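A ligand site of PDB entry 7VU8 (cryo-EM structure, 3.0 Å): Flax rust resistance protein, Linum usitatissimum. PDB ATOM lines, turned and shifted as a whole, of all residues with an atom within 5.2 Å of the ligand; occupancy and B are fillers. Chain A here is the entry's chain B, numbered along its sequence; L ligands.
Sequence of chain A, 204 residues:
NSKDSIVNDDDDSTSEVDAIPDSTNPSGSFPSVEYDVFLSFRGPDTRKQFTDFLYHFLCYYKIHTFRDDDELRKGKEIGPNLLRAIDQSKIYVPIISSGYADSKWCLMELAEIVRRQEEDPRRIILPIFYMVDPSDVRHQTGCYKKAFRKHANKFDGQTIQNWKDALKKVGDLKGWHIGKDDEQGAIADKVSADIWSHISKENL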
ATOM      1  N   PHE A  38      -8.179  18.149  19.916  1.00  0.00           N
ATOM      2  CA  PHE A  38      -7.738  17.053  20.777  1.00  0.00           C
ATOM      3  C   PHE A  38      -8.142  17.383  22.209  1.00  0.00           C
ATOM      4  O   PHE A  38      -7.767  18.444  22.717  1.00  0.00           O
ATOM      5  CB  PHE A  38      -6.237  16.848  20.671  1.00  0.00           C
ATOM      6  CG  PHE A  38      -5.679  15.885  21.674  1.00  0.00           C
ATOM      7  CD1 PHE A  38      -5.670  14.523  21.421  1.00  0.00           C
ATOM      8  CD2 PHE A  38      -5.148  16.330  22.869  1.00  0.00           C
ATOM      9  CE1 PHE A  38      -5.158  13.634  22.340  1.00  0.00           C
ATOM     10  CE2 PHE A  38      -4.636  15.450  23.790  1.00  0.00           C
ATOM     11  CZ  PHE A  38      -4.636  14.103  23.523  1.00  0.00           C
ATOM     12  N   LEU A  39      -8.880  16.488  22.842  1.00  0.00           N
ATOM     13  CA  LEU A  39      -9.398  16.736  24.179  1.00  0.00           C
ATOM     14  C   LEU A  39      -8.542  16.027  25.228  1.00  0.00           C
ATOM     15  O   LEU A  39      -7.558  15.353  24.916  1.00  0.00           O
ATOM     16  CB  LEU A  39     -10.854  16.272  24.270  1.00  0.00           C
ATOM     17  CG  LEU A  39     -11.926  17.258  23.805  1.00  0.00           C
ATOM     18  CD1 LEU A  39     -11.833  17.508  22.317  1.00  0.00           C
ATOM     19  CD2 LEU A  39     -13.291  16.729  24.163  1.00  0.00           C
ATOM     20  N   SER A  40      -8.928  16.210  26.486  1.00  0.00           N
ATOM     21  CA  SER A  40      -8.253  15.617  27.635  1.00  0.00           C
ATOM     22  C   SER A  40      -9.087  15.900  28.871  1.00  0.00           C
ATOM     23  O   SER A  40      -9.533  17.041  29.068  1.00  0.00           O
ATOM     24  CB  SER A  40      -6.841  16.186  27.822  1.00  0.00           C
ATOM     25  OG  SER A  40      -5.998  15.782  26.756  1.00  0.00           O
ATOM     26  N   PHE A  41      -9.341  14.885  29.693  1.00  0.00           N
ATOM     27  CA  PHE A  41     -10.251  15.088  30.858  1.00  0.00           C
ATOM     28  C   PHE A  41     -10.113  13.933  31.852  1.00  0.00           C
ATOM     29  O   PHE A  41      -9.190  13.103  31.709  1.00  0.00           O
ATOM     30  CB  PHE A  41     -11.700  15.161  30.380  1.00  0.00           C
ATOM     31  CG  PHE A  41     -12.117  14.054  29.446  1.00  0.00           C
ATOM     32  CD1 PHE A  41     -12.665  12.878  29.939  1.00  0.00           C
ATOM     33  CD2 PHE A  41     -11.981  14.184  28.069  1.00  0.00           C
ATOM     34  CE1 PHE A  41     -13.043  11.855  29.075  1.00  0.00           C
ATOM     35  CE2 PHE A  41     -12.353  13.159  27.213  1.00  0.00           C
ATOM     36  CZ  PHE A  41     -12.895  12.000  27.719  1.00  0.00           C
ATOM     37  N   ARG A  42     -11.012  13.876  32.841  1.00  0.00           N
ATOM     38  CA  ARG A  42     -11.020  12.774  33.834  1.00  0.00           C
ATOM     39  C   ARG A  42     -12.190  11.841  33.489  1.00  0.00           C
ATOM     40  O   ARG A  42     -13.347  12.313  33.565  1.00  0.00           O
ATOM     41  CB  ARG A  42     -11.166  13.345  35.249  1.00  0.00           C
ATOM     42  CG  ARG A  42     -10.780  12.383  36.353  1.00  0.00           C
ATOM     43  CD  ARG A  42      -9.311  11.987  36.289  1.00  0.00           C
ATOM     44  NE  ARG A  42      -8.843  11.417  37.544  1.00  0.00           N
ATOM     45  CZ  ARG A  42      -8.772  10.111  37.805  1.00  0.00           C
ATOM     46  NH1 ARG A  42      -9.121   9.231  36.888  1.00  0.00           N
ATOM     47  NH2 ARG A  42      -8.341   9.705  38.981  1.00  0.00           N
ATOM     48  N   GLY A  43     -11.913  10.585  33.126  1.00  0.00           N
ATOM     49  CA  GLY A  43     -12.982   9.673  32.697  1.00  0.00           C
ATOM     50  C   GLY A  43     -14.041   9.349  33.742  1.00  0.00           C
ATOM     51  O   GLY A  43     -15.226   9.387  33.376  1.00  0.00           O
ATOM     52  N   PRO A  44     -13.720   9.042  35.017  1.00  0.00           N
ATOM     53  CA  PRO A  44     -14.754   8.661  35.983  1.00  0.00           C
ATOM     54  C   PRO A  44     -15.781   9.760  36.291  1.00  0.00           C
ATOM     55  O   PRO A  44     -16.943   9.425  36.446  1.00  0.00           O
ATOM     56  CB  PRO A  44     -13.966   8.309  37.259  1.00  0.00           C
ATOM     57  CG  PRO A  44     -12.635   8.994  37.089  1.00  0.00           C
ATOM     58  CD  PRO A  44     -12.382   8.945  35.598  1.00  0.00           C
ATOM     59  N   ARG A  47     -16.520  11.926  31.676  1.00  0.00           N
ATOM     60  CA  ARG A  47     -16.338  11.295  30.332  1.00  0.00           C
ATOM     61  C   ARG A  47     -17.677  11.051  29.623  1.00  0.00           C
ATOM     62  O   ARG A  47     -17.772  11.375  28.425  1.00  0.00           O
ATOM     63  CB  ARG A  47     -15.609   9.951  30.446  1.00  0.00           C
ATOM     64  CG  ARG A  47     -15.501   9.160  29.156  1.00  0.00           C
ATOM     65  CD  ARG A  47     -14.586   7.961  29.335  1.00  0.00           C
ATOM     66  NE  ARG A  47     -13.190   8.353  29.497  1.00  0.00           N
ATOM     67  CZ  ARG A  47     -12.219   7.537  29.877  1.00  0.00           C
ATOM     68  NH1 ARG A  47     -12.480   6.273  30.159  1.00  0.00           N
ATOM     69  NH2 ARG A  47     -10.988   7.993  29.992  1.00  0.00           N
ATOM     70  N   PHE A  66     -11.314  14.365  18.098  1.00  0.00           N
ATOM     71  CA  PHE A  66     -10.753  13.068  18.568  1.00  0.00           C
ATOM     72  C   PHE A  66     -10.933  12.912  20.078  1.00  0.00           C
ATOM     73  O   PHE A  66     -10.552  13.837  20.826  1.00  0.00           O
ATOM     74  CB  PHE A  66      -9.275  12.945  18.193  1.00  0.00           C
ATOM     75  CG  PHE A  66      -8.576  11.752  18.797  1.00  0.00           C
ATOM     76  CD1 PHE A  66      -8.870  10.472  18.373  1.00  0.00           C
ATOM     77  CD2 PHE A  66      -7.635  11.909  19.805  1.00  0.00           C
ATOM     78  CE1 PHE A  66      -8.240   9.364  18.934  1.00  0.00           C
ATOM     79  CE2 PHE A  66      -7.004  10.812  20.368  1.00  0.00           C
ATOM     80  CZ  PHE A  66      -7.308   9.545  19.930  1.00  0.00           C
ATOM     81  N   ASP A  68     -10.517   9.690  23.221  1.00  0.00           N
ATOM     82  CA  ASP A  68     -10.128   8.283  23.504  1.00  0.00           C
ATOM     83  C   ASP A  68     -10.530   7.924  24.943  1.00  0.00           C
ATOM     84  O   ASP A  68     -10.580   8.842  25.777  1.00  0.00           O
ATOM     85  CB  ASP A  68      -8.640   8.046  23.225  1.00  0.00           C
ATOM     86  CG  ASP A  68      -8.259   6.572  23.115  1.00  0.00           C
ATOM     87  OD1 ASP A  68      -9.166   5.758  22.839  1.00  0.00           O
ATOM     88  OD2 ASP A  68      -7.074   6.261  23.322  1.00  0.00           O
ATOM     89  N   ASP A  69     -10.809   6.646  25.196  1.00  0.00           N
ATOM     90  CA  ASP A  69     -11.206   6.201  26.560  1.00  0.00           C
ATOM     91  C   ASP A  69     -10.285   5.058  26.996  1.00  0.00           C
ATOM     92  O   ASP A  69     -10.408   4.606  28.155  1.00  0.00           O
ATOM     93  CB  ASP A  69     -12.683   5.807  26.624  1.00  0.00           C
ATOM     94  CG  ASP A  69     -13.048   4.622  25.745  1.00  0.00           C
ATOM     95  OD1 ASP A  69     -12.348   4.391  24.734  1.00  0.00           O
ATOM     96  OD2 ASP A  69     -14.028   3.935  26.077  1.00  0.00           O
ATOM     97  N   ASP A  70      -9.422   4.598  26.086  1.00  0.00           N
ATOM     98  CA  ASP A  70      -8.493   3.474  26.387  1.00  0.00           C
ATOM     99  C   ASP A  70      -7.837   3.720  27.740  1.00  0.00           C
ATOM    100  O   ASP A  70      -7.205   4.775  27.907  1.00  0.00           O
ATOM    101  CB  ASP A  70      -7.449   3.288  25.286  1.00  0.00           C
ATOM    102  CG  ASP A  70      -8.044   2.868  23.955  1.00  0.00           C
ATOM    103  OD1 ASP A  70      -9.257   2.612  23.908  1.00  0.00           O
ATOM    104  OD2 ASP A  70      -7.273   2.789  22.976  1.00  0.00           O
ATOM    105  N   GLU A  71      -7.955   2.753  28.670  1.00  0.00           N
ATOM    106  CA  GLU A  71      -7.391   2.921  30.038  1.00  0.00           C
ATOM    107  C   GLU A  71      -5.862   2.761  29.999  1.00  0.00           C
ATOM    108  O   GLU A  71      -5.261   2.781  31.094  1.00  0.00           O
ATOM    109  CB  GLU A  71      -8.028   1.898  30.985  1.00  0.00           C
ATOM    110  CG  GLU A  71      -9.551   1.911  30.944  1.00  0.00           C
ATOM    111  CD  GLU A  71     -10.203   3.162  31.501  1.00  0.00           C
ATOM    112  OE1 GLU A  71      -9.661   3.729  32.465  1.00  0.00           O
ATOM    113  OE2 GLU A  71     -11.262   3.554  30.978  1.00  0.00           O
ATOM    114  N   LEU A  72      -5.277   2.643  28.799  1.00  0.00           N
ATOM    115  CA  LEU A  72      -3.797   2.516  28.630  1.00  0.00           C
ATOM    116  C   LEU A  72      -3.274   1.298  29.403  1.00  0.00           C
ATOM    117  O   LEU A  72      -3.773   0.187  29.122  1.00  0.00           O
ATOM    118  CB  LEU A  72      -3.120   3.823  29.080  1.00  0.00           C
ATOM    119  CG  LEU A  72      -1.617   3.907  28.782  1.00  0.00           C
ATOM    120  CD1 LEU A  72      -1.214   5.340  28.478  1.00  0.00           C
ATOM    121  CD2 LEU A  72      -0.807   3.363  29.942  1.00  0.00           C
ATOM    122  N   ARG A  73      -2.316   1.496  30.313  1.00  0.00           N
ATOM    123  CA  ARG A  73      -1.703   0.390  31.107  1.00  0.00           C
ATOM    124  C   ARG A  73      -0.940  -0.561  30.178  1.00  0.00           C
ATOM    125  O   ARG A  73      -0.433  -1.585  30.684  1.00  0.00           O
ATOM    126  CB  ARG A  73      -2.757  -0.316  31.973  1.00  0.00           C
ATOM    127  CG  ARG A  73      -3.446   0.603  32.979  1.00  0.00           C
ATOM    128  CD  ARG A  73      -4.839   0.138  33.336  1.00  0.00           C
ATOM    129  NE  ARG A  73      -5.601   1.190  33.997  1.00  0.00           N
ATOM    130  CZ  ARG A  73      -6.861   1.080  34.375  1.00  0.00           C
ATOM    131  NH1 ARG A  73      -7.481   2.097  34.959  1.00  0.00           N
ATOM    132  NH2 ARG A  73      -7.516  -0.056  34.165  1.00  0.00           N
ATOM    133  N   LEU A  82      -1.435   7.751  21.458  1.00  0.00           N
ATOM    134  CA  LEU A  82      -1.516   9.090  22.119  1.00  0.00           C
ATOM    135  C   LEU A  82      -0.482  10.062  21.547  1.00  0.00           C
ATOM    136  O   LEU A  82      -0.884  11.199  21.236  1.00  0.00           O
ATOM    137  CB  LEU A  82      -1.327   8.917  23.628  1.00  0.00           C
ATOM    138  CG  LEU A  82      -2.501   8.268  24.367  1.00  0.00           C
ATOM    139  CD1 LEU A  82      -2.168   8.091  25.841  1.00  0.00           C
ATOM    140  CD2 LEU A  82      -3.768   9.092  24.194  1.00  0.00           C
ATOM    141  N   TYR A 100      -8.391  16.090  38.503  1.00  0.00           N
ATOM    142  CA  TYR A 100      -7.436  16.072  37.371  1.00  0.00           C
ATOM    143  C   TYR A 100      -6.013  15.885  37.909  1.00  0.00           C
ATOM    144  O   TYR A 100      -5.075  15.902  37.091  1.00  0.00           O
ATOM    145  CB  TYR A 100      -7.577  17.336  36.532  1.00  0.00           C
ATOM    146  CG  TYR A 100      -7.105  17.206  35.097  1.00  0.00           C
ATOM    147  CD1 TYR A 100      -7.679  16.277  34.252  1.00  0.00           C
ATOM    148  CD2 TYR A 100      -6.099  18.011  34.596  1.00  0.00           C
ATOM    149  CE1 TYR A 100      -7.261  16.135  32.936  1.00  0.00           C
ATOM    150  CE2 TYR A 100      -5.672  17.889  33.278  1.00  0.00           C
ATOM    151  CZ  TYR A 100      -6.257  16.946  32.450  1.00  0.00           C
ATOM    152  OH  TYR A 100      -5.827  16.830  31.156  1.00  0.00           O
ATOM    153  N   SER A 103      -4.889  10.810  38.640  1.00  0.00           N
ATOM    154  CA  SER A 103      -4.546   9.801  37.603  1.00  0.00           C
ATOM    155  C   SER A 103      -3.071   9.931  37.249  1.00  0.00           C
ATOM    156  O   SER A 103      -2.609  11.058  37.007  1.00  0.00           O
ATOM    157  CB  SER A 103      -5.423   9.952  36.391  1.00  0.00           C
ATOM    158  OG  SER A 103      -4.965   9.134  35.331  1.00  0.00           O
ATOM    159  N   TRP A 105      -1.785   8.865  34.611  1.00  0.00           N
ATOM    160  CA  TRP A 105      -1.632   8.967  33.166  1.00  0.00           C
ATOM    161  C   TRP A 105      -1.913  10.380  32.680  1.00  0.00           C
ATOM    162  O   TRP A 105      -1.298  10.844  31.716  1.00  0.00           O
ATOM    163  CB  TRP A 105      -2.553   7.973  32.457  1.00  0.00           C
ATOM    164  CG  TRP A 105      -2.324   6.555  32.842  1.00  0.00           C
ATOM    165  CD1 TRP A 105      -3.211   5.718  33.453  1.00  0.00           C
ATOM    166  CD2 TRP A 105      -1.115   5.813  32.671  1.00  0.00           C
ATOM    167  NE1 TRP A 105      -2.632   4.488  33.660  1.00  0.00           N
ATOM    168  CE2 TRP A 105      -1.341   4.523  33.192  1.00  0.00           C
ATOM    169  CE3 TRP A 105       0.135   6.104  32.128  1.00  0.00           C
ATOM    170  CZ2 TRP A 105      -0.370   3.527  33.181  1.00  0.00           C
ATOM    171  CZ3 TRP A 105       1.107   5.117  32.119  1.00  0.00           C
ATOM    172  CH2 TRP A 105       0.846   3.850  32.644  1.00  0.00           C
ATOM    173  N   CYS A 106      -2.848  11.078  33.333  1.00  0.00           N
ATOM    174  CA  CYS A 106      -3.286  12.382  32.834  1.00  0.00           C
ATOM    175  C   CYS A 106      -2.155  13.404  32.885  1.00  0.00           C
ATOM    176  O   CYS A 106      -1.801  14.003  31.861  1.00  0.00           O
ATOM    177  CB  CYS A 106      -4.486  12.863  33.627  1.00  0.00           C
ATOM    178  SG  CYS A 106      -5.966  11.848  33.437  1.00  0.00           S
ATOM    179  N   GLU A 109       0.714  13.146  30.596  1.00  0.00           N
ATOM    180  CA  GLU A 109       0.273  13.488  29.249  1.00  0.00           C
ATOM    181  C   GLU A 109       0.124  14.982  29.090  1.00  0.00           C
ATOM    182  O   GLU A 109       0.435  15.541  28.033  1.00  0.00           O
ATOM    183  CB  GLU A 109      -1.031  12.763  28.937  1.00  0.00           C
ATOM    184  CG  GLU A 109      -1.507  12.929  27.516  1.00  0.00           C
ATOM    185  CD  GLU A 109      -2.332  14.176  27.316  1.00  0.00           C
ATOM    186  OE1 GLU A 109      -2.734  14.773  28.330  1.00  0.00           O
ATOM    187  OE2 GLU A 109      -2.565  14.554  26.150  1.00  0.00           O
ATOM    188  N   LEU A 110      -0.375  15.664  30.128  1.00  0.00           N
ATOM    189  CA  LEU A 110      -0.512  17.117  30.060  1.00  0.00           C
ATOM    190  C   LEU A 110       0.840  17.784  29.920  1.00  0.00           C
ATOM    191  O   LEU A 110       0.988  18.760  29.169  1.00  0.00           O
ATOM    192  CB  LEU A 110      -1.244  17.640  31.294  1.00  0.00           C
ATOM    193  CG  LEU A 110      -1.553  19.134  31.239  1.00  0.00           C
ATOM    194  CD1 LEU A 110      -2.471  19.422  30.068  1.00  0.00           C
ATOM    195  CD2 LEU A 110      -2.183  19.574  32.531  1.00  0.00           C
HETATM  196  O1  LIG L   1      -6.403  14.044  30.251  1.00  0.00           O
HETATM  197  P1  LIG L   1      -5.931  12.771  29.670  1.00  0.00           P
HETATM  198  O2  LIG L   1      -4.454  12.843  29.667  1.00  0.00           O
HETATM  199  O3  LIG L   1      -6.499  11.470  30.363  1.00  0.00           O
HETATM  200  O4  LIG L   1      -6.555  12.400  28.262  1.00  0.00           O
HETATM  201  C1  LIG L   1      -6.443  10.990  28.052  1.00  0.00           C
HETATM  202  C2  LIG L   1      -7.684  10.404  27.369  1.00  0.00           C
HETATM  203  O5  LIG L   1      -7.991   9.239  28.149  1.00  0.00           O
HETATM  204  C3  LIG L   1      -7.465  10.020  25.921  1.00  0.00           C
HETATM  205  O6  LIG L   1      -7.066  11.151  25.170  1.00  0.00           O
HETATM  206  C4  LIG L   1      -7.726   9.538  29.490  1.00  0.00           C
HETATM  207  N1  LIG L   1      -7.555   8.294  30.229  1.00  0.00           N
HETATM  208  C5  LIG L   1      -7.075   7.097  29.762  1.00  0.00           C
HETATM  209  N2  LIG L   1      -7.033   6.171  30.685  1.00  0.00           N
HETATM  210  C6  LIG L   1      -7.504   6.794  31.836  1.00  0.00           C
HETATM  211  C7  LIG L   1      -7.703   6.343  33.155  1.00  0.00           C
HETATM  212  N3  LIG L   1      -7.448   5.115  33.562  1.00  0.00           N
HETATM  213  N4  LIG L   1      -8.198   7.241  34.053  1.00  0.00           N
HETATM  214  C8  LIG L   1      -8.454   8.494  33.629  1.00  0.00           C
HETATM  215  N5  LIG L   1      -8.311   9.018  32.415  1.00  0.00           N
HETATM  216  C9  LIG L   1      -7.825   8.113  31.558  1.00  0.00           C
HETATM  217  C10 LIG L   1      -6.439  10.373  29.450  1.00  0.00           C
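SG of Cys 106 lies within hydrogen-bond range of O3 of the ligand, 3.1 Å away. N3 of the ligand sits at hydrogen-bond distance from OE1 of Glu 71. N of Phe 41 is in hydrogen-bond range of O1 of the ligand (3.1 Å). An oxygen (O1) of the ligand lies within hydrogen-bond range of the side-chain hydroxyl (OH) of Tyr 100 (3.0 Å). OE1 of Glu 109 lies close to O2 of the ligand, 2.9 Å away.
A nitrogen (N1) of the ligand sits close to the guanidinium group (NH2) of Arg 47, at 3.5 Å. N2 of the ligand lies close to O of Asp 70, 3.1 Å away. NH1 of Arg 73 lies close to N3 of the ligand (3.3 Å). Merely in contact with the ligand: Ser 40 (3.3 Å), Asp 68 (3.3 Å), Arg 42 (3.4 Å), Ser 103 (3.9 Å) and Gly 43 (3.99 Å). 13 residues have an atom within 4 Å of the ligand: Ser 40, Phe 41, Arg 42, Gly 43, Arg 47, Asp 68, Asp 70, Glu 71, Arg 73, Tyr 100, Ser 103, Cys 106 and Glu 109. The nearest printed residue that does not touch the ligand is Leu 82 (4.01 Å).
The backbone NH (N) of Asp 70 sits close to the side-chain carboxylate (OD1) of Asp 68 (3.5 Å). OE1 of Glu 71 lies within salt-bridge range of NH1 of Arg 73. The side-chain carboxylate of Glu 71 lies within salt-bridge range of the guanidinium group of Arg 47 (3.1 Å). The backbone carbonyl oxygen (O) of Asp 69 lies within hydrogen-bond range of the guanidinium group (NH1) of Arg 47. The side-chain sulfur of Cys 106 lies within hydrogen-bond range of the side-chain hydroxyl of Ser 103 (3.5 Å). OG of Ser 103 sits close to N of Trp 105, 3.3 Å away.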
